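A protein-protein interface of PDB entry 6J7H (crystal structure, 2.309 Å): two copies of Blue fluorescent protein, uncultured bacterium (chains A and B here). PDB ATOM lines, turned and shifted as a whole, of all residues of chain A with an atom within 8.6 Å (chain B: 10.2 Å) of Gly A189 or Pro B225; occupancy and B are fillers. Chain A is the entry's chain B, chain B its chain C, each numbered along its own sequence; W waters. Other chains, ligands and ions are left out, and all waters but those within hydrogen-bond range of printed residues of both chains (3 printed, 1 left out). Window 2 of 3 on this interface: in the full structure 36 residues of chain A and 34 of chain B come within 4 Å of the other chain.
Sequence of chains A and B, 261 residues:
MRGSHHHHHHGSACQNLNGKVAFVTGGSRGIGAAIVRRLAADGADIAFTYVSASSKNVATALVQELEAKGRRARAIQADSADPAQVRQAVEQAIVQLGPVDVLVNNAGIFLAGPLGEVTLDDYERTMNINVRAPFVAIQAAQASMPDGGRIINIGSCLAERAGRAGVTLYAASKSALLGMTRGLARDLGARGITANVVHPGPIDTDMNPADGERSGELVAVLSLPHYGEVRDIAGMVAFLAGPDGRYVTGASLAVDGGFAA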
ATOM      1  N   ASP A 147       6.533  -5.385  -2.398  1.00  0.00           N
ATOM      2  CA  ASP A 147       5.722  -4.262  -2.841  1.00  0.00           C
ATOM      3  C   ASP A 147       6.245  -3.739  -4.170  1.00  0.00           C
ATOM      4  O   ASP A 147       7.450  -3.740  -4.422  1.00  0.00           O
ATOM      5  CB  ASP A 147       5.739  -3.154  -1.789  1.00  0.00           C
ATOM      6  CG  ASP A 147       5.184  -3.614  -0.468  1.00  0.00           C
ATOM      7  OD1 ASP A 147       4.385  -4.577  -0.460  1.00  0.00           O
ATOM      8  OD2 ASP A 147       5.558  -3.027   0.568  1.00  0.00           O
ATOM      9  N   GLY A 148       5.325  -3.336  -5.045  1.00  0.00           N
ATOM     10  CA  GLY A 148       5.722  -2.924  -6.375  1.00  0.00           C
ATOM     11  C   GLY A 148       5.980  -4.047  -7.359  1.00  0.00           C
ATOM     12  O   GLY A 148       6.575  -3.793  -8.413  1.00  0.00           O
ATOM     13  N   GLY A 149       5.569  -5.282  -7.044  1.00  0.00           N
ATOM     14  CA  GLY A 149       5.752  -6.412  -7.940  1.00  0.00           C
ATOM     15  C   GLY A 149       4.787  -6.388  -9.118  1.00  0.00           C
ATOM     16  O   GLY A 149       3.853  -5.587  -9.194  1.00  0.00           O
ATOM     17  N   ARG A 182      -8.392  -8.782 -13.469  1.00  0.00           N
ATOM     18  CA  ARG A 182      -9.030  -7.618 -12.860  1.00  0.00           C
ATOM     19  C   ARG A 182      -9.225  -7.812 -11.358  1.00  0.00           C
ATOM     20  O   ARG A 182      -9.001  -6.885 -10.571  1.00  0.00           O
ATOM     21  CB  ARG A 182     -10.362  -7.326 -13.566  1.00  0.00           C
ATOM     22  CG  ARG A 182     -10.180  -6.632 -14.926  1.00  0.00           C
ATOM     23  CD  ARG A 182     -11.501  -6.173 -15.585  1.00  0.00           C
ATOM     24  NE  ARG A 182     -12.367  -7.258 -16.047  1.00  0.00           N
ATOM     25  CZ  ARG A 182     -12.397  -7.706 -17.302  1.00  0.00           C
ATOM     26  NH1 ARG A 182     -11.615  -7.158 -18.225  1.00  0.00           N
ATOM     27  NH2 ARG A 182     -13.215  -8.690 -17.644  1.00  0.00           N
ATOM     28  N   GLY A 183      -9.590  -9.023 -10.935  1.00  0.00           N
ATOM     29  CA  GLY A 183      -9.702  -9.280  -9.508  1.00  0.00           C
ATOM     30  C   GLY A 183      -8.352  -9.243  -8.813  1.00  0.00           C
ATOM     31  O   GLY A 183      -8.239  -8.775  -7.674  1.00  0.00           O
ATOM     32  N   LEU A 184      -7.302  -9.720  -9.494  1.00  0.00           N
ATOM     33  CA  LEU A 184      -5.978  -9.661  -8.891  1.00  0.00           C
ATOM     34  C   LEU A 184      -5.532  -8.227  -8.693  1.00  0.00           C
ATOM     35  O   LEU A 184      -4.885  -7.921  -7.684  1.00  0.00           O
ATOM     36  CB  LEU A 184      -4.958 -10.408  -9.750  1.00  0.00           C
ATOM     37  CG  LEU A 184      -5.089 -11.927  -9.727  1.00  0.00           C
ATOM     38  CD1 LEU A 184      -4.170 -12.530 -10.757  1.00  0.00           C
ATOM     39  CD2 LEU A 184      -4.791 -12.455  -8.339  1.00  0.00           C
ATOM     40  N   ALA A 185      -5.903  -7.333  -9.619  1.00  0.00           N
ATOM     41  CA  ALA A 185      -5.537  -5.926  -9.481  1.00  0.00           C
ATOM     42  C   ALA A 185      -6.171  -5.312  -8.243  1.00  0.00           C
ATOM     43  O   ALA A 185      -5.542  -4.503  -7.549  1.00  0.00           O
ATOM     44  CB  ALA A 185      -5.954  -5.149 -10.734  1.00  0.00           C
ATOM     45  N   ARG A 186      -7.421  -5.675  -7.960  1.00  0.00           N
ATOM     46  CA  ARG A 186      -8.068  -5.241  -6.729  1.00  0.00           C
ATOM     47  C   ARG A 186      -7.469  -5.950  -5.526  1.00  0.00           C
ATOM     48  O   ARG A 186      -7.258  -5.328  -4.479  1.00  0.00           O
ATOM     49  CB  ARG A 186      -9.572  -5.505  -6.799  1.00  0.00           C
ATOM     50  CG  ARG A 186     -10.291  -4.669  -7.835  1.00  0.00           C
ATOM     51  CD  ARG A 186     -10.361  -3.208  -7.415  1.00  0.00           C
ATOM     52  NE  ARG A 186     -10.982  -2.381  -8.446  1.00  0.00           N
ATOM     53  CZ  ARG A 186     -11.167  -1.071  -8.349  1.00  0.00           C
ATOM     54  NH1 ARG A 186     -10.785  -0.418  -7.263  1.00  0.00           N
ATOM     55  NH2 ARG A 186     -11.719  -0.409  -9.346  1.00  0.00           N
ATOM     56  N   ASP A 187      -7.171  -7.247  -5.661  1.00  0.00           N
ATOM     57  CA  ASP A 187      -6.668  -7.984  -4.506  1.00  0.00           C
ATOM     58  C   ASP A 187      -5.299  -7.483  -4.055  1.00  0.00           C
ATOM     59  O   ASP A 187      -5.039  -7.419  -2.849  1.00  0.00           O
ATOM     60  CB  ASP A 187      -6.602  -9.489  -4.793  1.00  0.00           C
ATOM     61  CG  ASP A 187      -7.934 -10.207  -4.525  1.00  0.00           C
ATOM     62  OD1 ASP A 187      -8.680  -9.798  -3.604  1.00  0.00           O
ATOM     63  OD2 ASP A 187      -8.204 -11.237  -5.185  1.00  0.00           O
ATOM     64  N   LEU A 188      -4.436  -7.062  -4.982  1.00  0.00           N
ATOM     65  CA  LEU A 188      -3.044  -6.775  -4.637  1.00  0.00           C
ATOM     66  C   LEU A 188      -2.635  -5.312  -4.798  1.00  0.00           C
ATOM     67  O   LEU A 188      -1.467  -4.973  -4.527  1.00  0.00           O
ATOM     68  CB  LEU A 188      -2.117  -7.680  -5.464  1.00  0.00           C
ATOM     69  CG  LEU A 188      -2.421  -9.164  -5.223  1.00  0.00           C
ATOM     70  CD1 LEU A 188      -1.714 -10.085  -6.213  1.00  0.00           C
ATOM     71  CD2 LEU A 188      -2.006  -9.521  -3.805  1.00  0.00           C
ATOM     72  N   GLY A 189      -3.559  -4.426  -5.176  1.00  0.00           N
ATOM     73  CA  GLY A 189      -3.182  -3.043  -5.435  1.00  0.00           C
ATOM     74  C   GLY A 189      -2.685  -2.301  -4.209  1.00  0.00           C
ATOM     75  O   GLY A 189      -1.822  -1.425  -4.318  1.00  0.00           O
ATOM     76  N   ALA A 190      -3.193  -2.651  -3.026  1.00  0.00           N
ATOM     77  CA  ALA A 190      -2.783  -1.959  -1.807  1.00  0.00           C
ATOM     78  C   ALA A 190      -1.292  -2.142  -1.518  1.00  0.00           C
ATOM     79  O   ALA A 190      -0.685  -1.312  -0.833  1.00  0.00           O
ATOM     80  CB  ALA A 190      -3.618  -2.443  -0.622  1.00  0.00           C
ATOM     81  N   ARG A 191      -0.700  -3.238  -1.980  1.00  0.00           N
ATOM     82  CA  ARG A 191       0.733  -3.464  -1.870  1.00  0.00           C
ATOM     83  C   ARG A 191       1.517  -2.867  -3.043  1.00  0.00           C
ATOM     84  O   ARG A 191       2.743  -3.000  -3.079  1.00  0.00           O
ATOM     85  CB  ARG A 191       1.022  -4.976  -1.733  1.00  0.00           C
ATOM     86  CG  ARG A 191       0.550  -5.626  -0.390  1.00  0.00           C
ATOM     87  CD  ARG A 191       0.313  -7.158  -0.497  1.00  0.00           C
ATOM     88  NE  ARG A 191       1.522  -7.898  -0.847  1.00  0.00           N
ATOM     89  CZ  ARG A 191       1.570  -9.195  -1.158  1.00  0.00           C
ATOM     90  NH1 ARG A 191       0.466  -9.940  -1.185  1.00  0.00           N
ATOM     91  NH2 ARG A 191       2.738  -9.750  -1.455  1.00  0.00           N
ATOM     92  N   GLY A 192       0.849  -2.209  -4.000  1.00  0.00           N
ATOM     93  CA  GLY A 192       1.551  -1.659  -5.148  1.00  0.00           C
ATOM     94  C   GLY A 192       1.827  -2.655  -6.249  1.00  0.00           C
ATOM     95  O   GLY A 192       2.567  -2.343  -7.191  1.00  0.00           O
ATOM     96  N   ILE A 193       1.292  -3.863  -6.129  1.00  0.00           N
ATOM     97  CA  ILE A 193       1.465  -4.886  -7.145  1.00  0.00           C
ATOM     98  C   ILE A 193       0.464  -4.638  -8.268  1.00  0.00           C
ATOM     99  O   ILE A 193      -0.730  -4.440  -8.025  1.00  0.00           O
ATOM    100  CB  ILE A 193       1.298  -6.281  -6.518  1.00  0.00           C
ATOM    101  CG1 ILE A 193       2.377  -6.497  -5.454  1.00  0.00           C
ATOM    102  CG2 ILE A 193       1.366  -7.383  -7.577  1.00  0.00           C
ATOM    103  CD1 ILE A 193       2.138  -7.719  -4.562  1.00  0.00           C
ATOM    104  N   THR A 194       0.947  -4.651  -9.502  1.00  0.00           N
ATOM    105  CA  THR A 194       0.095  -4.521 -10.670  1.00  0.00           C
ATOM    106  C   THR A 194      -0.197  -5.907 -11.221  1.00  0.00           C
ATOM    107  O   THR A 194       0.578  -6.853 -11.022  1.00  0.00           O
ATOM    108  CB  THR A 194       0.753  -3.663 -11.753  1.00  0.00           C
ATOM    109  OG1 THR A 194       1.777  -4.416 -12.421  1.00  0.00           O
ATOM    110  CG2 THR A 194       1.380  -2.420 -11.144  1.00  0.00           C
ATOM    111  N   ALA A 195      -1.329  -6.027 -11.906  1.00  0.00           N
ATOM    112  CA  ALA A 195      -1.724  -7.272 -12.555  1.00  0.00           C
ATOM    113  C   ALA A 195      -2.324  -6.929 -13.910  1.00  0.00           C
ATOM    114  O   ALA A 195      -3.317  -6.200 -13.973  1.00  0.00           O
ATOM    115  CB  ALA A 195      -2.726  -8.044 -11.689  1.00  0.00           C
ATOM    116  N   ARG A 246       4.385   1.183 -13.775  1.00  0.00           N
ATOM    117  CA  ARG A 246       4.074   1.294 -12.355  1.00  0.00           C
ATOM    118  C   ARG A 246       2.606   1.635 -12.094  1.00  0.00           C
ATOM    119  O   ARG A 246       2.033   1.197 -11.086  1.00  0.00           O
ATOM    120  CB  ARG A 246       4.984   2.394 -11.797  1.00  0.00           C
ATOM    121  CG  ARG A 246       5.275   2.430 -10.327  1.00  0.00           C
ATOM    122  CD  ARG A 246       6.317   3.529 -10.056  1.00  0.00           C
ATOM    123  NE  ARG A 246       5.778   4.889 -10.178  1.00  0.00           N
ATOM    124  CZ  ARG A 246       5.861   5.655 -11.268  1.00  0.00           C
ATOM    125  NH1 ARG A 246       6.460   5.198 -12.360  1.00  0.00           N
ATOM    126  NH2 ARG A 246       5.354   6.884 -11.268  1.00  0.00           N
ATOM    127  N   TYR A 247       1.976   2.390 -12.994  1.00  0.00           N
ATOM    128  CA  TYR A 247       0.603   2.841 -12.813  1.00  0.00           C
ATOM    129  C   TYR A 247      -0.389   2.134 -13.741  1.00  0.00           C
ATOM    130  O   TYR A 247      -1.547   2.568 -13.839  1.00  0.00           O
ATOM    131  CB  TYR A 247       0.533   4.365 -12.979  1.00  0.00           C
ATOM    132  CG  TYR A 247      -0.633   5.015 -12.263  1.00  0.00           C
ATOM    133  CD1 TYR A 247      -0.769   4.928 -10.879  1.00  0.00           C
ATOM    134  CD2 TYR A 247      -1.606   5.702 -12.976  1.00  0.00           C
ATOM    135  CE1 TYR A 247      -1.840   5.523 -10.227  1.00  0.00           C
ATOM    136  CE2 TYR A 247      -2.673   6.294 -12.342  1.00  0.00           C
ATOM    137  CZ  TYR A 247      -2.793   6.207 -10.969  1.00  0.00           C
ATOM    138  OH  TYR A 247      -3.884   6.805 -10.351  1.00  0.00           O
ATOM    139  N   THR A 249      -2.477  -1.152 -14.260  1.00  0.00           N
ATOM    140  CA  THR A 249      -2.926  -2.361 -13.575  1.00  0.00           C
ATOM    141  C   THR A 249      -4.386  -2.643 -13.916  1.00  0.00           C
ATOM    142  O   THR A 249      -5.179  -1.721 -14.124  1.00  0.00           O
ATOM    143  CB  THR A 249      -2.722  -2.232 -12.058  1.00  0.00           C
ATOM    144  OG1 THR A 249      -3.040  -3.472 -11.416  1.00  0.00           O
ATOM    145  CG2 THR A 249      -3.586  -1.124 -11.488  1.00  0.00           C
ATOM    146  N   PRO B 202      -6.548   9.261 -12.823  1.00  0.00           N
ATOM    147  CA  PRO B 202      -6.184  10.483 -12.105  1.00  0.00           C
ATOM    148  C   PRO B 202      -4.686  10.704 -12.200  1.00  0.00           C
ATOM    149  O   PRO B 202      -3.888   9.805 -11.912  1.00  0.00           O
ATOM    150  CB  PRO B 202      -6.617  10.193 -10.663  1.00  0.00           C
ATOM    151  CG  PRO B 202      -7.536   9.017 -10.752  1.00  0.00           C
ATOM    152  CD  PRO B 202      -7.079   8.223 -11.928  1.00  0.00           C
ATOM    153  N   ALA B 210      -3.566  16.376  -6.764  1.00  0.00           N
ATOM    154  CA  ALA B 210      -3.806  15.209  -5.925  1.00  0.00           C
ATOM    155  C   ALA B 210      -4.246  15.610  -4.522  1.00  0.00           C
ATOM    156  O   ALA B 210      -4.707  14.755  -3.758  1.00  0.00           O
ATOM    157  CB  ALA B 210      -2.558  14.324  -5.851  1.00  0.00           C
ATOM    158  N   SER B 215     -10.067  14.703  -4.498  1.00  0.00           N
ATOM    159  CA  SER B 215      -9.062  13.662  -4.695  1.00  0.00           C
ATOM    160  C   SER B 215      -9.399  12.394  -3.917  1.00  0.00           C
ATOM    161  O   SER B 215      -9.128  11.281  -4.381  1.00  0.00           O
ATOM    162  CB  SER B 215      -7.698  14.193  -4.260  1.00  0.00           C
ATOM    163  OG  SER B 215      -7.314  15.309  -5.040  1.00  0.00           O
ATOM    164  N   GLY B 216     -10.001  12.542  -2.737  1.00  0.00           N
ATOM    165  CA  GLY B 216     -10.271  11.381  -1.905  1.00  0.00           C
ATOM    166  C   GLY B 216     -11.347  10.480  -2.477  1.00  0.00           C
ATOM    167  O   GLY B 216     -11.289   9.254  -2.325  1.00  0.00           O
ATOM    168  N   GLU B 217     -12.353  11.068  -3.127  1.00  0.00           N
ATOM    169  CA  GLU B 217     -13.363  10.238  -3.768  1.00  0.00           C
ATOM    170  C   GLU B 217     -12.758   9.417  -4.902  1.00  0.00           C
ATOM    171  O   GLU B 217     -13.128   8.252  -5.093  1.00  0.00           O
ATOM    172  CB  GLU B 217     -14.512  11.103  -4.288  1.00  0.00           C
ATOM    173  CG  GLU B 217     -14.416  11.373  -5.783  1.00  0.00           C
ATOM    174  CD  GLU B 217     -15.570  12.171  -6.317  1.00  0.00           C
ATOM    175  OE1 GLU B 217     -16.394  12.624  -5.502  1.00  0.00           O
ATOM    176  OE2 GLU B 217     -15.647  12.341  -7.552  1.00  0.00           O
ATOM    177  N   LEU B 218     -11.785   9.982  -5.634  1.00  0.00           N
ATOM    178  CA  LEU B 218     -11.197   9.229  -6.738  1.00  0.00           C
ATOM    179  C   LEU B 218     -10.285   8.126  -6.238  1.00  0.00           C
ATOM    180  O   LEU B 218     -10.373   6.988  -6.710  1.00  0.00           O
ATOM    181  CB  LEU B 218     -10.393  10.148  -7.665  1.00  0.00           C
ATOM    182  CG  LEU B 218     -11.170  10.803  -8.813  1.00  0.00           C
ATOM    183  CD1 LEU B 218     -10.337  11.830  -9.605  1.00  0.00           C
ATOM    184  CD2 LEU B 218     -11.821   9.763  -9.751  1.00  0.00           C
ATOM    185  N   VAL B 219      -9.441   8.437  -5.255  1.00  0.00           N
ATOM    186  CA  VAL B 219      -8.462   7.470  -4.778  1.00  0.00           C
ATOM    187  C   VAL B 219      -9.143   6.251  -4.178  1.00  0.00           C
ATOM    188  O   VAL B 219      -8.689   5.120  -4.377  1.00  0.00           O
ATOM    189  CB  VAL B 219      -7.529   8.169  -3.775  1.00  0.00           C
ATOM    190  CG1 VAL B 219      -6.760   7.156  -2.954  1.00  0.00           C
ATOM    191  CG2 VAL B 219      -6.584   9.112  -4.508  1.00  0.00           C
ATOM    192  N   ALA B 220     -10.291   6.447  -3.525  1.00  0.00           N
ATOM    193  CA  ALA B 220     -10.986   5.347  -2.861  1.00  0.00           C
ATOM    194  C   ALA B 220     -11.476   4.289  -3.847  1.00  0.00           C
ATOM    195  O   ALA B 220     -11.632   3.122  -3.468  1.00  0.00           O
ATOM    196  CB  ALA B 220     -12.161   5.895  -2.048  1.00  0.00           C
ATOM    197  N   VAL B 221     -11.775   4.678  -5.095  1.00  0.00           N
ATOM    198  CA  VAL B 221     -12.250   3.735  -6.106  1.00  0.00           C
ATOM    199  C   VAL B 221     -11.130   3.174  -6.986  1.00  0.00           C
ATOM    200  O   VAL B 221     -11.409   2.373  -7.886  1.00  0.00           O
ATOM    201  CB  VAL B 221     -13.352   4.378  -6.982  1.00  0.00           C
ATOM    202  CG1 VAL B 221     -14.462   4.941  -6.115  1.00  0.00           C
ATOM    203  CG2 VAL B 221     -12.781   5.458  -7.892  1.00  0.00           C
ATOM    204  N   LEU B 222      -9.881   3.590  -6.777  1.00  0.00           N
ATOM    205  CA  LEU B 222      -8.736   3.057  -7.509  1.00  0.00           C
ATOM    206  C   LEU B 222      -8.294   1.712  -6.936  1.00  0.00           C
ATOM    207  O   LEU B 222      -8.596   1.364  -5.791  1.00  0.00           O
ATOM    208  CB  LEU B 222      -7.555   4.031  -7.468  1.00  0.00           C
ATOM    209  CG  LEU B 222      -7.767   5.436  -8.030  1.00  0.00           C
ATOM    210  CD1 LEU B 222      -6.516   6.279  -7.867  1.00  0.00           C
ATOM    211  CD2 LEU B 222      -8.211   5.386  -9.499  1.00  0.00           C
ATOM    212  N   SER B 223      -7.616   0.921  -7.781  1.00  0.00           N
ATOM    213  CA  SER B 223      -6.914  -0.267  -7.293  1.00  0.00           C
ATOM    214  C   SER B 223      -5.598   0.098  -6.604  1.00  0.00           C
ATOM    215  O   SER B 223      -5.262  -0.470  -5.559  1.00  0.00           O
ATOM    216  CB  SER B 223      -6.668  -1.242  -8.441  1.00  0.00           C
ATOM    217  OG  SER B 223      -7.888  -1.719  -8.983  1.00  0.00           O
ATOM    218  N   LEU B 224      -4.831   1.025  -7.183  1.00  0.00           N
ATOM    219  CA  LEU B 224      -3.670   1.600  -6.513  1.00  0.00           C
ATOM    220  C   LEU B 224      -4.097   2.883  -5.814  1.00  0.00           C
ATOM    221  O   LEU B 224      -4.539   3.821  -6.491  1.00  0.00           O
ATOM    222  CB  LEU B 224      -2.559   1.898  -7.503  1.00  0.00           C
ATOM    223  CG  LEU B 224      -2.009   0.733  -8.326  1.00  0.00           C
ATOM    224  CD1 LEU B 224      -1.083   1.255  -9.404  1.00  0.00           C
ATOM    225  CD2 LEU B 224      -1.292  -0.249  -7.433  1.00  0.00           C
ATOM    226  N   PRO B 225      -3.963   2.984  -4.495  1.00  0.00           N
ATOM    227  CA  PRO B 225      -4.595   4.077  -3.736  1.00  0.00           C
ATOM    228  C   PRO B 225      -3.847   5.408  -3.795  1.00  0.00           C
ATOM    229  O   PRO B 225      -3.509   5.998  -2.768  1.00  0.00           O
ATOM    230  CB  PRO B 225      -4.639   3.508  -2.313  1.00  0.00           C
ATOM    231  CG  PRO B 225      -3.435   2.629  -2.237  1.00  0.00           C
ATOM    232  CD  PRO B 225      -3.190   2.082  -3.626  1.00  0.00           C
ATOM    233  N   HIS B 226      -3.565   5.878  -5.011  1.00  0.00           N
ATOM    234  CA  HIS B 226      -2.898   7.161  -5.173  1.00  0.00           C
ATOM    235  C   HIS B 226      -3.073   7.626  -6.611  1.00  0.00           C
ATOM    236  O   HIS B 226      -3.325   6.825  -7.514  1.00  0.00           O
ATOM    237  CB  HIS B 226      -1.412   7.061  -4.816  1.00  0.00           C
ATOM    238  CG  HIS B 226      -0.670   6.051  -5.630  1.00  0.00           C
ATOM    239  ND1 HIS B 226      -0.066   6.364  -6.829  1.00  0.00           N
ATOM    240  CD2 HIS B 226      -0.469   4.725  -5.444  1.00  0.00           C
ATOM    241  CE1 HIS B 226       0.499   5.281  -7.332  1.00  0.00           C
ATOM    242  NE2 HIS B 226       0.268   4.272  -6.511  1.00  0.00           N
ATOM    243  N   TYR B 227      -2.926   8.934  -6.807  1.00  0.00           N
ATOM    244  CA  TYR B 227      -2.877   9.511  -8.143  1.00  0.00           C
ATOM    245  C   TYR B 227      -1.612   9.071  -8.876  1.00  0.00           C
ATOM    246  O   TYR B 227      -0.593   8.753  -8.260  1.00  0.00           O
ATOM    247  CB  TYR B 227      -2.918  11.036  -8.056  1.00  0.00           C
ATOM    248  CG  TYR B 227      -4.297  11.635  -8.044  1.00  0.00           C
ATOM    249  CD1 TYR B 227      -5.311  11.088  -7.268  1.00  0.00           C
ATOM    250  CD2 TYR B 227      -4.576  12.783  -8.771  1.00  0.00           C
ATOM    251  CE1 TYR B 227      -6.571  11.644  -7.245  1.00  0.00           C
ATOM    252  CE2 TYR B 227      -5.837  13.353  -8.750  1.00  0.00           C
ATOM    253  CZ  TYR B 227      -6.828  12.781  -7.985  1.00  0.00           C
ATOM    254  OH  TYR B 227      -8.082  13.348  -7.972  1.00  0.00           O
ATOM    255  N   GLY B 228      -1.695   9.031 -10.208  1.00  0.00           N
ATOM    256  CA  GLY B 228      -0.526   8.833 -11.041  1.00  0.00           C
ATOM    257  C   GLY B 228       0.222  10.136 -11.277  1.00  0.00           C
ATOM    258  O   GLY B 228      -0.178  11.207 -10.827  1.00  0.00           O
ATOM    259  N   ASP B 256      -4.417   3.932 -15.522  1.00  0.00           N
ATOM    260  CA  ASP B 256      -5.440   4.507 -14.656  1.00  0.00           C
ATOM    261  C   ASP B 256      -5.378   4.056 -13.204  1.00  0.00           C
ATOM    262  O   ASP B 256      -6.346   4.283 -12.469  1.00  0.00           O
ATOM    263  CB  ASP B 256      -6.841   4.216 -15.217  1.00  0.00           C
ATOM    264  CG  ASP B 256      -7.201   2.717 -15.220  1.00  0.00           C
ATOM    265  OD1 ASP B 256      -6.339   1.850 -14.952  1.00  0.00           O
ATOM    266  OD2 ASP B 256      -8.386   2.414 -15.472  1.00  0.00           O
ATOM    267  N   GLY B 257      -4.332   3.341 -12.787  1.00  0.00           N
ATOM    268  CA  GLY B 257      -4.285   2.909 -11.400  1.00  0.00           C
ATOM    269  C   GLY B 257      -5.338   1.891 -11.024  1.00  0.00           C
ATOM    270  O   GLY B 257      -5.686   1.767  -9.844  1.00  0.00           O
ATOM    271  N   GLY B 258      -5.858   1.148 -11.996  1.00  0.00           N
ATOM    272  CA  GLY B 258      -6.926   0.219 -11.708  1.00  0.00           C
ATOM    273  C   GLY B 258      -8.298   0.837 -11.559  1.00  0.00           C
ATOM    274  O   GLY B 258      -9.150   0.242 -10.897  1.00  0.00           O
ATOM    275  N   PHE B 259      -8.535   2.026 -12.133  1.00  0.00           N
ATOM    276  CA  PHE B 259      -9.862   2.645 -12.077  1.00  0.00           C
ATOM    277  C   PHE B 259     -10.906   1.756 -12.727  1.00  0.00           C
ATOM    278  O   PHE B 259     -12.027   1.631 -12.219  1.00  0.00           O
ATOM    279  CB  PHE B 259      -9.831   4.004 -12.788  1.00  0.00           C
ATOM    280  CG  PHE B 259     -11.188   4.649 -12.972  1.00  0.00           C
ATOM    281  CD1 PHE B 259     -11.733   5.463 -11.986  1.00  0.00           C
ATOM    282  CD2 PHE B 259     -11.913   4.453 -14.142  1.00  0.00           C
ATOM    283  CE1 PHE B 259     -12.979   6.074 -12.164  1.00  0.00           C
ATOM    284  CE2 PHE B 259     -13.166   5.055 -14.331  1.00  0.00           C
ATOM    285  CZ  PHE B 259     -13.698   5.865 -13.344  1.00  0.00           C
HETATM  286  O   HOH W   1     -13.081   2.542  -9.741  1.00  0.00           O
HETATM  287  O   HOH W   2      -7.128  -0.574 -15.675  1.00  0.00           O
HETATM  288  O   HOH W   3      -4.190   1.169 -15.832  1.00  0.00           O
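No position is printed for both chains. Of the 24 pairs that touch across the chains among the printed residues, none has its exchanged pair printed and touching as well.
Hydrophobic or aromatic side chains of chain B within 4 Å of the printed part of chain A: Pro B202, Leu B222, Leu B224, Pro B225 and His B226.
Of the printed residues of chain B, Ala A185 touches Ser B223. Leu A188 touches none of the printed residues of chain B. Ala A190 touches just one residue of chain B: Ser B223. Printed residues of chain A within 4 Å of Val B221: Arg A186. Printed residues of chain A within 4 Å of Leu B224: Gly A189 (3.4 Å), Gly A192 (3.9 Å), Arg A246 (3.5 Å), Tyr A247 (3.97 Å) and Thr A249 (3.99 Å). Of the printed residues of chain A, Pro B225 touches Gly A189 (3.8 Å). Of the printed residues of chain A, Tyr B227 touches Tyr A247 (3.5 Å). Of the printed residues of chain A, Gly B228 touches Tyr A247. Printed residues of chain A within 4 Å of Phe B259: Arg A186. The nearest residue of chain A that does not touch Pro B225 is Ala A190 (4.5 Å). The nearest printed residue of chain A that does not touch Gly B258 is Tyr A247 (4.9 Å).
Water W3 lies within hydrogen-bond range of OD1 of Asp B256 (2.4 Å) and N of Thr A249 (3.3 Å). Water W1 lies within hydrogen-bond range of O of Val B221, O of Phe B259 and NH2 of Arg A186. Water W2 bridges OD1 of Asp B256 (2.6 Å) and O of Thr A249 (2.7 Å).
Ser B223 touches Ala A185 (CB to O, 3.6 Å). NH2 of Arg A186 touches O of Phe B259, 3.5 Å away. Ser B223 touches Gly A189 (O to CA, 3.3 Å). Leu B224 touches Gly A189. O of Gly A189 touches CD of Pro B225 (3.8 Å). Leu B224 touches Gly A192 (CD2 to CA, 3.9 Å). Tyr A247 touches Leu B222. O of Tyr A247 touches N of Asp B256 (3.6 Å). Asp B256 touches Thr A249 (OD1 to O, 3.8 Å). CG2 of Thr A249 touches C of Gly B257, at 3.5 Å.
The side-chain carboxylate of Asp B256 is in hydrogen-bond range of the backbone NH of Phe B259 (3.4 Å). The side-chain carboxylate (OD1) of Asp B256 lies within hydrogen-bond range of the backbone NH (N) of Gly B258, at 3.1 Å. The backbone carbonyl oxygen of Pro B202 lies within hydrogen-bond range of the backbone NH of Gly B228. O of Gly B257 is in hydrogen-bond range of N of Leu B224 (2.9 Å). The backbone NH (N) of Ala A195 is in hydrogen-bond range of the side-chain hydroxyl (OG1) of Thr A249. N of Ser B223 is in hydrogen-bond range of O of Gly B257, at 2.9 Å.
O of Tyr A247 is in hydrogen-bond range of N of Gly B257 (3.1 Å). OH of Tyr A247 sits close to N of Gly B228 (3.1 Å). The side-chain hydroxyl of Tyr A247 is in hydrogen-bond range of the backbone carbonyl oxygen of Pro B202, 3.4 Å away. NH1 of Arg A186 lies within hydrogen-bond range of O of Val B221 (2.9 Å). The side-chain hydroxyl of Ser B223 lies within hydrogen-bond range of the guanidinium group of Arg A186. The backbone carbonyl oxygen (O) of Gly B258 lies within hydrogen-bond range of the guanidinium group (NH2) of Arg A186 (3.1 Å). O of His B226 is in hydrogen-bond range of OH of Tyr A247, at 2.9 Å. The guanidinium group (NH1) of Arg A186 lies within hydrogen-bond range of the backbone carbonyl oxygen (O) of Leu B222, 3.2 Å away.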
